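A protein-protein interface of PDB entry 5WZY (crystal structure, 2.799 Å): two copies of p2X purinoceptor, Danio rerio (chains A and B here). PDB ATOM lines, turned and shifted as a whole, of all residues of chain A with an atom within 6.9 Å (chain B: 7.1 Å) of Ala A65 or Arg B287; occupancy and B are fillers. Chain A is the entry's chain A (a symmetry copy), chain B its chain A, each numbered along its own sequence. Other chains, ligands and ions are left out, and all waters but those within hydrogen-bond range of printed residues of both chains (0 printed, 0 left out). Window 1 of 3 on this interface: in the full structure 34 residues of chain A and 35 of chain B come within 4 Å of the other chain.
The side-chain carboxylate (OE1) of Glu B285 is in salt-bridge range of the guanidinium group (NH2) of Arg A60, 3.6 Å away. The indole nitrogen (NE1) of Trp B142 is in hydrogen-bond range of the side-chain carboxylate (OD2) of Asp A66 (2.8 Å). OH of Tyr B277 is in hydrogen-bond range of O of Ala A65 (3.0 Å). OD2 of Asp A66 lies within salt-bridge range of NH1 of Arg B287 (3.3 Å). OH of Tyr B277 sits at hydrogen-bond distance from OD1 of Asp A66. OD2 of Asp A63 lies within salt-bridge range of NH2 of Arg B287 (2.9 Å). The side-chain amide oxygen (OE1) of Gln B91 lies within hydrogen-bond range of the backbone NH (N) of Ile A61 (2.7 Å).
The backbone NH (N) of Ala A65 is in hydrogen-bond range of the side-chain carboxylate (OD1) of Asp A63 (2.9 Å). The guanidinium group of Arg B287 sits at hydrogen-bond distance from the side-chain amide oxygen of Gln B89 (2.7 Å). OD2 of Asp A66 sits at hydrogen-bond distance from N of Asp A63 (2.6 Å). O of Phe B274 sits at hydrogen-bond distance from N of Ile B290 (2.8 Å). NH1 of Arg A60 lies within salt-bridge range of OD1 of Asp A66 (3.9 Å). The indole nitrogen (NE1) of Trp B142 sits close to the side-chain amide nitrogen (NE2) of Gln B91 (3.5 Å).
Among the printed residues, merely in contact across the chains: Asp A63 with Trp B142 (3.1 Å), Arg A60 with Gln B91 (3.3 Å), Arg A60 with Trp B142 (3.4 Å), Ile A61 with Trp B142 (3.4 Å), Pro A71 with Phe B274 (3.7 Å), Val A64 with Arg B273 (3.8 Å), Pro A71 with Arg B273 (3.8 Å), Ala A65 with Ala B275 (3.8 Å), Ala A65 with Arg B287 (3.9 Å), Ile A61 with Ser B141 (3.9 Å) and Ala A65 with Phe B274 (3.9 Å).
Of chain B, only Phe B274, Ala B275, Tyr B277 and Arg B287 come within 4 Å of Ala A65. Printed residues of chain A within 4 Å of Arg B287: Asp A63 (2.9 Å), Ala A65 (3.9 Å) and Asp A66 (3.3 Å). Printed residues of chain A within 4 Å of Tyr B277: Ala A65 (3.0 Å) and Asp A66 (2.8 Å). Of the printed residues of chain A, Phe B274 touches Ala A65 and Pro A71. Of the printed residues of chain B, Val A64 touches Arg B273. Of the printed residues of chain A, Trp B142 touches Arg A60 (3.4 Å), Ile A61 (3.4 Å), Asp A63 (3.1 Å) and Asp A66 (2.8 Å). The nearest residue of chain B that does not touch Ala A65 is Leu B289 (4.04 Å). The nearest residue of chain A that does not touch Arg B287 is Val A64 (5.9 Å). The nearest printed residue of chain A that does not touch Gln B91 is Trp A62 (4.9 Å).
Of the 23 printed residues of chain B, 9 touch a printed residue of chain A. Along chain B the printed residues that touch a printed residue of chain A span positions 91 to 287. Of the 12 printed residues of chain A, 7 touch a printed residue of chain B. Printed residues of chain A that touch a printed residue of chain B: Arg A60, Ile A61, Asp A63, Val A64, Ala A65, Asp A66 and Pro A71. Hydrophobic or aromatic side chains of chain A that line the printed part of chain B: Ile A61, Val A64, Ala A65 and Pro A71.
No position is printed for both chains.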
ATOM      1  N   GLY A  48     -28.691 -25.887  21.994  1.00  0.00           N
ATOM      2  CA  GLY A  48     -29.120 -26.281  23.322  1.00  0.00           C
ATOM      3  C   GLY A  48     -27.978 -26.340  24.316  1.00  0.00           C
ATOM      4  O   GLY A  48     -26.808 -26.290  23.935  1.00  0.00           O
ATOM      5  N   ARG A  60     -21.743 -28.774  35.665  1.00  0.00           N
ATOM      6  CA  ARG A  60     -21.119 -28.599  34.358  1.00  0.00           C
ATOM      7  C   ARG A  60     -22.163 -28.321  33.244  1.00  0.00           C
ATOM      8  O   ARG A  60     -23.218 -28.961  33.193  1.00  0.00           O
ATOM      9  CB  ARG A  60     -20.296 -29.867  34.059  1.00  0.00           C
ATOM     10  CG  ARG A  60     -18.986 -29.650  33.326  1.00  0.00           C
ATOM     11  CD  ARG A  60     -19.190 -29.728  31.807  1.00  0.00           C
ATOM     12  NE  ARG A  60     -17.948 -29.509  31.060  1.00  0.00           N
ATOM     13  CZ  ARG A  60     -17.892 -29.203  29.765  1.00  0.00           C
ATOM     14  NH1 ARG A  60     -19.012 -29.076  29.068  1.00  0.00           N
ATOM     15  NH2 ARG A  60     -16.716 -29.018  29.167  1.00  0.00           N
ATOM     16  N   ILE A  61     -21.890 -27.366  32.357  1.00  0.00           N
ATOM     17  CA  ILE A  61     -22.762 -27.190  31.188  1.00  0.00           C
ATOM     18  C   ILE A  61     -22.095 -27.575  29.857  1.00  0.00           C
ATOM     19  O   ILE A  61     -20.917 -27.294  29.631  1.00  0.00           O
ATOM     20  CB  ILE A  61     -23.388 -25.759  31.084  1.00  0.00           C
ATOM     21  CG1 ILE A  61     -22.393 -24.767  30.502  1.00  0.00           C
ATOM     22  CG2 ILE A  61     -23.901 -25.279  32.417  1.00  0.00           C
ATOM     23  CD1 ILE A  61     -22.694 -24.431  29.077  1.00  0.00           C
ATOM     24  N   TRP A  62     -22.875 -28.212  28.987  1.00  0.00           N
ATOM     25  CA  TRP A  62     -22.421 -28.660  27.677  1.00  0.00           C
ATOM     26  C   TRP A  62     -23.179 -27.899  26.601  1.00  0.00           C
ATOM     27  O   TRP A  62     -24.405 -28.013  26.504  1.00  0.00           O
ATOM     28  CB  TRP A  62     -22.659 -30.168  27.523  1.00  0.00           C
ATOM     29  CG  TRP A  62     -21.867 -30.969  28.497  1.00  0.00           C
ATOM     30  CD1 TRP A  62     -22.080 -31.066  29.839  1.00  0.00           C
ATOM     31  CD2 TRP A  62     -20.708 -31.765  28.217  1.00  0.00           C
ATOM     32  NE1 TRP A  62     -21.128 -31.874  30.412  1.00  0.00           N
ATOM     33  CE2 TRP A  62     -20.272 -32.313  29.437  1.00  0.00           C
ATOM     34  CE3 TRP A  62     -19.992 -32.066  27.052  1.00  0.00           C
ATOM     35  CZ2 TRP A  62     -19.159 -33.138  29.526  1.00  0.00           C
ATOM     36  CZ3 TRP A  62     -18.885 -32.891  27.146  1.00  0.00           C
ATOM     37  CH2 TRP A  62     -18.487 -33.422  28.370  1.00  0.00           C
ATOM     38  N   ASP A  63     -22.474 -27.090  25.814  1.00  0.00           N
ATOM     39  CA  ASP A  63     -23.135 -26.452  24.685  1.00  0.00           C
ATOM     40  C   ASP A  63     -22.732 -27.103  23.389  1.00  0.00           C
ATOM     41  O   ASP A  63     -22.072 -28.131  23.408  1.00  0.00           O
ATOM     42  CB  ASP A  63     -23.020 -24.920  24.651  1.00  0.00           C
ATOM     43  CG  ASP A  63     -21.632 -24.414  24.315  1.00  0.00           C
ATOM     44  OD1 ASP A  63     -20.894 -25.019  23.510  1.00  0.00           O
ATOM     45  OD2 ASP A  63     -21.294 -23.350  24.851  1.00  0.00           O
ATOM     46  N   VAL A  64     -23.171 -26.515  22.278  1.00  0.00           N
ATOM     47  CA  VAL A  64     -23.006 -27.109  20.964  1.00  0.00           C
ATOM     48  C   VAL A  64     -21.555 -27.474  20.674  1.00  0.00           C
ATOM     49  O   VAL A  64     -21.283 -28.520  20.080  1.00  0.00           O
ATOM     50  CB  VAL A  64     -23.560 -26.182  19.878  1.00  0.00           C
ATOM     51  CG1 VAL A  64     -22.642 -25.019  19.643  1.00  0.00           C
ATOM     52  CG2 VAL A  64     -23.772 -26.932  18.614  1.00  0.00           C
ATOM     53  N   ALA A  65     -20.618 -26.639  21.117  1.00  0.00           N
ATOM     54  CA  ALA A  65     -19.225 -26.893  20.816  1.00  0.00           C
ATOM     55  C   ALA A  65     -18.667 -27.996  21.715  1.00  0.00           C
ATOM     56  O   ALA A  65     -17.590 -28.530  21.456  1.00  0.00           O
ATOM     57  CB  ALA A  65     -18.401 -25.617  20.925  1.00  0.00           C
ATOM     58  N   ASP A  66     -19.378 -28.304  22.789  1.00  0.00           N
ATOM     59  CA  ASP A  66     -19.011 -29.415  23.657  1.00  0.00           C
ATOM     60  C   ASP A  66     -19.546 -30.770  23.162  1.00  0.00           C
ATOM     61  O   ASP A  66     -18.848 -31.787  23.241  1.00  0.00           O
ATOM     62  CB  ASP A  66     -19.419 -29.157  25.120  1.00  0.00           C
ATOM     63  CG  ASP A  66     -18.981 -27.770  25.634  1.00  0.00           C
ATOM     64  OD1 ASP A  66     -17.761 -27.535  25.748  1.00  0.00           O
ATOM     65  OD2 ASP A  66     -19.860 -26.917  25.945  1.00  0.00           O
ATOM     66  N   TYR A  67     -20.791 -30.795  22.696  1.00  0.00           N
ATOM     67  CA  TYR A  67     -21.449 -32.059  22.337  1.00  0.00           C
ATOM     68  C   TYR A  67     -21.539 -32.463  20.839  1.00  0.00           C
ATOM     69  O   TYR A  67     -22.146 -33.491  20.512  1.00  0.00           O
ATOM     70  CB  TYR A  67     -22.821 -32.212  23.045  1.00  0.00           C
ATOM     71  CG  TYR A  67     -23.808 -31.114  22.734  1.00  0.00           C
ATOM     72  CD1 TYR A  67     -24.349 -30.989  21.467  1.00  0.00           C
ATOM     73  CD2 TYR A  67     -24.210 -30.203  23.713  1.00  0.00           C
ATOM     74  CE1 TYR A  67     -25.232 -29.992  21.168  1.00  0.00           C
ATOM     75  CE2 TYR A  67     -25.115 -29.191  23.426  1.00  0.00           C
ATOM     76  CZ  TYR A  67     -25.618 -29.098  22.144  1.00  0.00           C
ATOM     77  OH  TYR A  67     -26.508 -28.115  21.805  1.00  0.00           O
ATOM     78  N   ILE A  68     -20.999 -31.666  19.924  1.00  0.00           N
ATOM     79  CA  ILE A  68     -21.035 -32.083  18.526  1.00  0.00           C
ATOM     80  C   ILE A  68     -19.629 -32.424  18.006  1.00  0.00           C
ATOM     81  O   ILE A  68     -18.770 -31.539  17.864  1.00  0.00           O
ATOM     82  CB  ILE A  68     -21.740 -31.047  17.640  1.00  0.00           C
ATOM     83  CG1 ILE A  68     -23.188 -30.871  18.102  1.00  0.00           C
ATOM     84  CG2 ILE A  68     -21.696 -31.466  16.165  1.00  0.00           C
ATOM     85  CD1 ILE A  68     -24.096 -31.995  17.706  1.00  0.00           C
ATOM     86  N   ILE A  69     -19.394 -33.717  17.783  1.00  0.00           N
ATOM     87  CA  ILE A  69     -18.071 -34.244  17.438  1.00  0.00           C
ATOM     88  C   ILE A  69     -18.050 -34.968  16.092  1.00  0.00           C
ATOM     89  O   ILE A  69     -18.689 -35.997  15.948  1.00  0.00           O
ATOM     90  CB  ILE A  69     -17.610 -35.272  18.479  1.00  0.00           C
ATOM     91  CG1 ILE A  69     -18.117 -34.933  19.893  1.00  0.00           C
ATOM     92  CG2 ILE A  69     -16.117 -35.460  18.403  1.00  0.00           C
ATOM     93  CD1 ILE A  69     -17.498 -33.730  20.520  1.00  0.00           C
ATOM     94  N   PRO A  71     -17.277 -30.789  14.769  1.00  0.00           N
ATOM     95  CA  PRO A  71     -18.284 -29.720  14.748  1.00  0.00           C
ATOM     96  C   PRO A  71     -19.025 -29.630  13.435  1.00  0.00           C
ATOM     97  O   PRO A  71     -20.082 -29.009  13.361  1.00  0.00           O
ATOM     98  CB  PRO A  71     -17.456 -28.461  14.939  1.00  0.00           C
ATOM     99  CG  PRO A  71     -16.106 -28.941  15.399  1.00  0.00           C
ATOM    100  CD  PRO A  71     -15.912 -30.243  14.781  1.00  0.00           C
ATOM    101  N   THR B  86     -15.008 -15.511  20.786  1.00  0.00           N
ATOM    102  CA  THR B  86     -15.222 -15.151  22.169  1.00  0.00           C
ATOM    103  C   THR B  86     -14.206 -15.914  22.984  1.00  0.00           C
ATOM    104  O   THR B  86     -14.267 -17.139  23.051  1.00  0.00           O
ATOM    105  CB  THR B  86     -16.627 -15.576  22.617  1.00  0.00           C
ATOM    106  OG1 THR B  86     -17.593 -14.851  21.858  1.00  0.00           O
ATOM    107  CG2 THR B  86     -16.834 -15.320  24.102  1.00  0.00           C
ATOM    108  N   THR B  87     -13.322 -15.204  23.671  1.00  0.00           N
ATOM    109  CA  THR B  87     -12.205 -15.857  24.343  1.00  0.00           C
ATOM    110  C   THR B  87     -12.370 -15.796  25.850  1.00  0.00           C
ATOM    111  O   THR B  87     -13.191 -15.038  26.364  1.00  0.00           O
ATOM    112  CB  THR B  87     -10.837 -15.220  23.978  1.00  0.00           C
ATOM    113  OG1 THR B  87     -10.762 -13.896  24.519  1.00  0.00           O
ATOM    114  CG2 THR B  87     -10.643 -15.162  22.471  1.00  0.00           C
ATOM    115  N   ASN B  88     -11.628 -16.652  26.537  1.00  0.00           N
ATOM    116  CA  ASN B  88     -11.541 -16.634  27.988  1.00  0.00           C
ATOM    117  C   ASN B  88     -12.846 -17.054  28.676  1.00  0.00           C
ATOM    118  O   ASN B  88     -13.134 -16.658  29.809  1.00  0.00           O
ATOM    119  CB  ASN B  88     -11.053 -15.261  28.452  1.00  0.00           C
ATOM    120  CG  ASN B  88     -10.518 -15.269  29.863  1.00  0.00           C
ATOM    121  OD1 ASN B  88     -10.012 -16.288  30.358  1.00  0.00           O
ATOM    122  ND2 ASN B  88     -10.627 -14.120  30.528  1.00  0.00           N
ATOM    123  N   GLN B  89     -13.623 -17.896  28.006  1.00  0.00           N
ATOM    124  CA  GLN B  89     -14.850 -18.408  28.600  1.00  0.00           C
ATOM    125  C   GLN B  89     -14.567 -19.370  29.748  1.00  0.00           C
ATOM    126  O   GLN B  89     -13.639 -20.155  29.669  1.00  0.00           O
ATOM    127  CB  GLN B  89     -15.671 -19.130  27.550  1.00  0.00           C
ATOM    128  CG  GLN B  89     -16.133 -18.253  26.438  1.00  0.00           C
ATOM    129  CD  GLN B  89     -17.261 -18.898  25.681  1.00  0.00           C
ATOM    130  OE1 GLN B  89     -17.218 -20.095  25.377  1.00  0.00           O
ATOM    131  NE2 GLN B  89     -18.299 -18.129  25.406  1.00  0.00           N
ATOM    132  N   THR B  90     -15.366 -19.314  30.812  1.00  0.00           N
ATOM    133  CA  THR B  90     -15.269 -20.311  31.884  1.00  0.00           C
ATOM    134  C   THR B  90     -16.652 -20.703  32.348  1.00  0.00           C
ATOM    135  O   THR B  90     -17.601 -19.940  32.152  1.00  0.00           O
ATOM    136  CB  THR B  90     -14.505 -19.787  33.115  1.00  0.00           C
ATOM    137  OG1 THR B  90     -15.028 -18.512  33.486  1.00  0.00           O
ATOM    138  CG2 THR B  90     -13.011 -19.666  32.827  1.00  0.00           C
ATOM    139  N   GLN B  91     -16.771 -21.860  33.003  1.00  0.00           N
ATOM    140  CA  GLN B  91     -18.085 -22.290  33.474  1.00  0.00           C
ATOM    141  C   GLN B  91     -18.377 -21.459  34.689  1.00  0.00           C
ATOM    142  O   GLN B  91     -17.731 -21.603  35.730  1.00  0.00           O
ATOM    143  CB  GLN B  91     -18.078 -23.755  33.881  1.00  0.00           C
ATOM    144  CG  GLN B  91     -17.796 -24.691  32.735  1.00  0.00           C
ATOM    145  CD  GLN B  91     -19.006 -25.481  32.315  1.00  0.00           C
ATOM    146  OE1 GLN B  91     -19.878 -25.783  33.139  1.00  0.00           O
ATOM    147  NE2 GLN B  91     -19.072 -25.830  31.029  1.00  0.00           N
ATOM    148  N   SER B 141     -23.358 -20.880  32.543  1.00  0.00           N
ATOM    149  CA  SER B 141     -23.007 -21.007  31.131  1.00  0.00           C
ATOM    150  C   SER B 141     -21.493 -20.909  30.946  1.00  0.00           C
ATOM    151  O   SER B 141     -20.747 -20.755  31.930  1.00  0.00           O
ATOM    152  CB  SER B 141     -23.672 -19.874  30.357  1.00  0.00           C
ATOM    153  OG  SER B 141     -23.712 -20.145  28.980  1.00  0.00           O
ATOM    154  N   TRP B 142     -21.037 -20.979  29.695  1.00  0.00           N
ATOM    155  CA  TRP B 142     -19.658 -20.598  29.404  1.00  0.00           C
ATOM    156  C   TRP B 142     -19.659 -19.084  29.246  1.00  0.00           C
ATOM    157  O   TRP B 142     -20.171 -18.547  28.253  1.00  0.00           O
ATOM    158  CB  TRP B 142     -19.153 -21.211  28.086  1.00  0.00           C
ATOM    159  CG  TRP B 142     -18.915 -22.695  28.059  1.00  0.00           C
ATOM    160  CD1 TRP B 142     -19.766 -23.654  27.577  1.00  0.00           C
ATOM    161  CD2 TRP B 142     -17.736 -23.390  28.491  1.00  0.00           C
ATOM    162  NE1 TRP B 142     -19.198 -24.905  27.705  1.00  0.00           N
ATOM    163  CE2 TRP B 142     -17.948 -24.767  28.250  1.00  0.00           C
ATOM    164  CE3 TRP B 142     -16.523 -22.986  29.059  1.00  0.00           C
ATOM    165  CZ2 TRP B 142     -16.991 -25.733  28.556  1.00  0.00           C
ATOM    166  CZ3 TRP B 142     -15.575 -23.947  29.357  1.00  0.00           C
ATOM    167  CH2 TRP B 142     -15.815 -25.304  29.112  1.00  0.00           C
ATOM    168  N   CYS B 143     -19.008 -18.401  30.179  1.00  0.00           N
ATOM    169  CA  CYS B 143     -19.121 -16.949  30.292  1.00  0.00           C
ATOM    170  C   CYS B 143     -17.755 -16.279  30.200  1.00  0.00           C
ATOM    171  O   CYS B 143     -16.766 -16.771  30.763  1.00  0.00           O
ATOM    172  CB  CYS B 143     -19.790 -16.559  31.629  1.00  0.00           C
ATOM    173  SG  CYS B 143     -21.554 -17.053  31.898  1.00  0.00           S
ATOM    174  N   PRO B 144     -17.693 -15.120  29.541  1.00  0.00           N
ATOM    175  CA  PRO B 144     -18.765 -14.319  28.945  1.00  0.00           C
ATOM    176  C   PRO B 144     -19.426 -14.943  27.730  1.00  0.00           C
ATOM    177  O   PRO B 144     -18.829 -15.791  27.082  1.00  0.00           O
ATOM    178  CB  PRO B 144     -18.041 -13.040  28.518  1.00  0.00           C
ATOM    179  CG  PRO B 144     -16.639 -13.399  28.434  1.00  0.00           C
ATOM    180  CD  PRO B 144     -16.407 -14.412  29.485  1.00  0.00           C
ATOM    181  N   ARG B 273     -20.257 -23.480  15.275  1.00  0.00           N
ATOM    182  CA  ARG B 273     -19.489 -23.101  16.440  1.00  0.00           C
ATOM    183  C   ARG B 273     -18.537 -24.242  16.794  1.00  0.00           C
ATOM    184  O   ARG B 273     -18.884 -25.418  16.654  1.00  0.00           O
ATOM    185  CB  ARG B 273     -20.425 -22.756  17.602  1.00  0.00           C
ATOM    186  CG  ARG B 273     -20.701 -21.258  17.729  1.00  0.00           C
ATOM    187  CD  ARG B 273     -21.866 -20.926  18.658  1.00  0.00           C
ATOM    188  NE  ARG B 273     -23.081 -20.794  17.873  1.00  0.00           N
ATOM    189  CZ  ARG B 273     -23.610 -19.631  17.496  1.00  0.00           C
ATOM    190  NH1 ARG B 273     -23.044 -18.487  17.858  1.00  0.00           N
ATOM    191  NH2 ARG B 273     -24.721 -19.616  16.765  1.00  0.00           N
ATOM    192  N   PHE B 274     -17.325 -23.889  17.211  1.00  0.00           N
ATOM    193  CA  PHE B 274     -16.336 -24.866  17.664  1.00  0.00           C
ATOM    194  C   PHE B 274     -15.455 -24.235  18.734  1.00  0.00           C
ATOM    195  O   PHE B 274     -15.445 -23.021  18.894  1.00  0.00           O
ATOM    196  CB  PHE B 274     -15.527 -25.477  16.497  1.00  0.00           C
ATOM    197  CG  PHE B 274     -14.609 -24.514  15.794  1.00  0.00           C
ATOM    198  CD1 PHE B 274     -15.089 -23.659  14.816  1.00  0.00           C
ATOM    199  CD2 PHE B 274     -13.252 -24.483  16.092  1.00  0.00           C
ATOM    200  CE1 PHE B 274     -14.234 -22.770  14.161  1.00  0.00           C
ATOM    201  CE2 PHE B 274     -12.395 -23.609  15.446  1.00  0.00           C
ATOM    202  CZ  PHE B 274     -12.885 -22.747  14.478  1.00  0.00           C
ATOM    203  N   ALA B 275     -14.746 -25.044  19.505  1.00  0.00           N
ATOM    204  CA  ALA B 275     -14.049 -24.468  20.644  1.00  0.00           C
ATOM    205  C   ALA B 275     -12.635 -24.989  20.748  1.00  0.00           C
ATOM    206  O   ALA B 275     -12.322 -26.032  20.190  1.00  0.00           O
ATOM    207  CB  ALA B 275     -14.813 -24.743  21.928  1.00  0.00           C
ATOM    208  N   LYS B 276     -11.785 -24.250  21.446  1.00  0.00           N
ATOM    209  CA  LYS B 276     -10.476 -24.733  21.813  1.00  0.00           C
ATOM    210  C   LYS B 276     -10.417 -24.674  23.322  1.00  0.00           C
ATOM    211  O   LYS B 276     -10.852 -23.689  23.902  1.00  0.00           O
ATOM    212  CB  LYS B 276      -9.394 -23.862  21.194  1.00  0.00           C
ATOM    213  CG  LYS B 276      -9.440 -23.850  19.697  1.00  0.00           C
ATOM    214  CD  LYS B 276      -8.064 -23.649  19.103  1.00  0.00           C
ATOM    215  CE  LYS B 276      -7.733 -22.172  18.975  1.00  0.00           C
ATOM    216  NZ  LYS B 276      -6.775 -21.921  17.842  1.00  0.00           N
ATOM    217  N   TYR B 277      -9.913 -25.730  23.963  1.00  0.00           N
ATOM    218  CA  TYR B 277      -9.931 -25.790  25.422  1.00  0.00           C
ATOM    219  C   TYR B 277      -8.545 -25.692  26.016  1.00  0.00           C
ATOM    220  O   TYR B 277      -7.591 -26.206  25.445  1.00  0.00           O
ATOM    221  CB  TYR B 277     -10.636 -27.054  25.917  1.00  0.00           C
ATOM    222  CG  TYR B 277     -12.029 -27.239  25.363  1.00  0.00           C
ATOM    223  CD1 TYR B 277     -12.227 -27.848  24.135  1.00  0.00           C
ATOM    224  CD2 TYR B 277     -13.142 -26.802  26.056  1.00  0.00           C
ATOM    225  CE1 TYR B 277     -13.494 -28.021  23.609  1.00  0.00           C
ATOM    226  CE2 TYR B 277     -14.409 -26.972  25.540  1.00  0.00           C
ATOM    227  CZ  TYR B 277     -14.583 -27.582  24.310  1.00  0.00           C
ATOM    228  OH  TYR B 277     -15.849 -27.768  23.778  1.00  0.00           O
ATOM    229  N   TYR B 278      -8.456 -25.031  27.168  1.00  0.00           N
ATOM    230  CA  TYR B 278      -7.204 -24.805  27.888  1.00  0.00           C
ATOM    231  C   TYR B 278      -7.400 -25.026  29.385  1.00  0.00           C
ATOM    232  O   TYR B 278      -8.491 -24.827  29.905  1.00  0.00           O
ATOM    233  CB  TYR B 278      -6.737 -23.361  27.688  1.00  0.00           C
ATOM    234  CG  TYR B 278      -6.721 -22.904  26.256  1.00  0.00           C
ATOM    235  CD1 TYR B 278      -5.664 -23.238  25.402  1.00  0.00           C
ATOM    236  CD2 TYR B 278      -7.756 -22.142  25.749  1.00  0.00           C
ATOM    237  CE1 TYR B 278      -5.645 -22.824  24.070  1.00  0.00           C
ATOM    238  CE2 TYR B 278      -7.751 -21.728  24.414  1.00  0.00           C
ATOM    239  CZ  TYR B 278      -6.691 -22.064  23.583  1.00  0.00           C
ATOM    240  OH  TYR B 278      -6.703 -21.631  22.271  1.00  0.00           O
ATOM    241  N   THR B 284      -8.371 -24.752  36.065  1.00  0.00           N
ATOM    242  CA  THR B 284      -9.802 -24.741  35.770  1.00  0.00           C
ATOM    243  C   THR B 284      -9.973 -24.445  34.280  1.00  0.00           C
ATOM    244  O   THR B 284      -9.385 -23.498  33.743  1.00  0.00           O
ATOM    245  CB  THR B 284     -10.612 -23.711  36.639  1.00  0.00           C
ATOM    246  OG1 THR B 284     -10.643 -22.430  35.998  1.00  0.00           O
ATOM    247  CG2 THR B 284     -10.021 -23.564  38.051  1.00  0.00           C
ATOM    248  N   GLU B 285     -10.771 -25.272  33.614  1.00  0.00           N
ATOM    249  CA  GLU B 285     -10.962 -25.138  32.178  1.00  0.00           C
ATOM    250  C   GLU B 285     -11.452 -23.764  31.739  1.00  0.00           C
ATOM    251  O   GLU B 285     -12.488 -23.265  32.184  1.00  0.00           O
ATOM    252  CB  GLU B 285     -11.926 -26.201  31.666  1.00  0.00           C
ATOM    253  CG  GLU B 285     -11.241 -27.327  30.940  1.00  0.00           C
ATOM    254  CD  GLU B 285     -12.127 -27.948  29.874  1.00  0.00           C
ATOM    255  OE1 GLU B 285     -13.375 -27.784  29.940  1.00  0.00           O
ATOM    256  OE2 GLU B 285     -11.565 -28.601  28.963  1.00  0.00           O
ATOM    257  N   THR B 286     -10.686 -23.163  30.845  1.00  0.00           N
ATOM    258  CA  THR B 286     -11.128 -21.984  30.145  1.00  0.00           C
ATOM    259  C   THR B 286     -11.138 -22.324  28.649  1.00  0.00           C
ATOM    260  O   THR B 286     -10.433 -23.219  28.216  1.00  0.00           O
ATOM    261  CB  THR B 286     -10.268 -20.764  30.515  1.00  0.00           C
ATOM    262  OG1 THR B 286      -9.717 -20.169  29.336  1.00  0.00           O
ATOM    263  CG2 THR B 286      -9.162 -21.173  31.466  1.00  0.00           C
ATOM    264  N   ARG B 287     -11.962 -21.640  27.867  1.00  0.00           N
ATOM    265  CA  ARG B 287     -12.288 -22.101  26.528  1.00  0.00           C
ATOM    266  C   ARG B 287     -12.378 -20.913  25.592  1.00  0.00           C
ATOM    267  O   ARG B 287     -12.782 -19.836  26.011  1.00  0.00           O
ATOM    268  CB  ARG B 287     -13.641 -22.796  26.590  1.00  0.00           C
ATOM    269  CG  ARG B 287     -14.149 -23.340  25.277  1.00  0.00           C
ATOM    270  CD  ARG B 287     -15.563 -23.889  25.425  1.00  0.00           C
ATOM    271  NE  ARG B 287     -16.565 -22.874  25.141  1.00  0.00           N
ATOM    272  CZ  ARG B 287     -17.798 -23.151  24.748  1.00  0.00           C
ATOM    273  NH1 ARG B 287     -18.165 -24.413  24.582  1.00  0.00           N
ATOM    274  NH2 ARG B 287     -18.646 -22.171  24.499  1.00  0.00           N
ATOM    275  N   THR B 288     -11.985 -21.099  24.338  1.00  0.00           N
ATOM    276  CA  THR B 288     -12.210 -20.095  23.308  1.00  0.00           C
ATOM    277  C   THR B 288     -13.269 -20.645  22.394  1.00  0.00           C
ATOM    278  O   THR B 288     -13.153 -21.774  21.918  1.00  0.00           O
ATOM    279  CB  THR B 288     -10.965 -19.817  22.432  1.00  0.00           C
ATOM    280  OG1 THR B 288      -9.929 -19.217  23.214  1.00  0.00           O
ATOM    281  CG2 THR B 288     -11.324 -18.877  21.290  1.00  0.00           C
ATOM    282  N   LEU B 289     -14.304 -19.854  22.139  1.00  0.00           N
ATOM    283  CA  LEU B 289     -15.370 -20.266  21.242  1.00  0.00           C
ATOM    284  C   LEU B 289     -15.300 -19.485  19.936  1.00  0.00           C
ATOM    285  O   LEU B 289     -15.110 -18.268  19.939  1.00  0.00           O
ATOM    286  CB  LEU B 289     -16.712 -20.046  21.929  1.00  0.00           C
ATOM    287  CG  LEU B 289     -17.968 -20.146  21.078  1.00  0.00           C
ATOM    288  CD1 LEU B 289     -18.277 -21.589  20.700  1.00  0.00           C
ATOM    289  CD2 LEU B 289     -19.087 -19.509  21.858  1.00  0.00           C
ATOM    290  N   ILE B 290     -15.414 -20.183  18.816  1.00  0.00           N
ATOM    291  CA  ILE B 290     -15.460 -19.520  17.526  1.00  0.00           C
ATOM    292  C   ILE B 290     -16.785 -19.841  16.852  1.00  0.00           C
ATOM    293  O   ILE B 290     -17.168 -21.011  16.735  1.00  0.00           O
ATOM    294  CB  ILE B 290     -14.301 -19.944  16.565  1.00  0.00           C
ATOM    295  CG1 ILE B 290     -12.935 -19.517  17.091  1.00  0.00           C
ATOM    296  CG2 ILE B 290     -14.479 -19.316  15.199  1.00  0.00           C
ATOM    297  CD1 ILE B 290     -12.272 -20.575  17.903  1.00  0.00           C
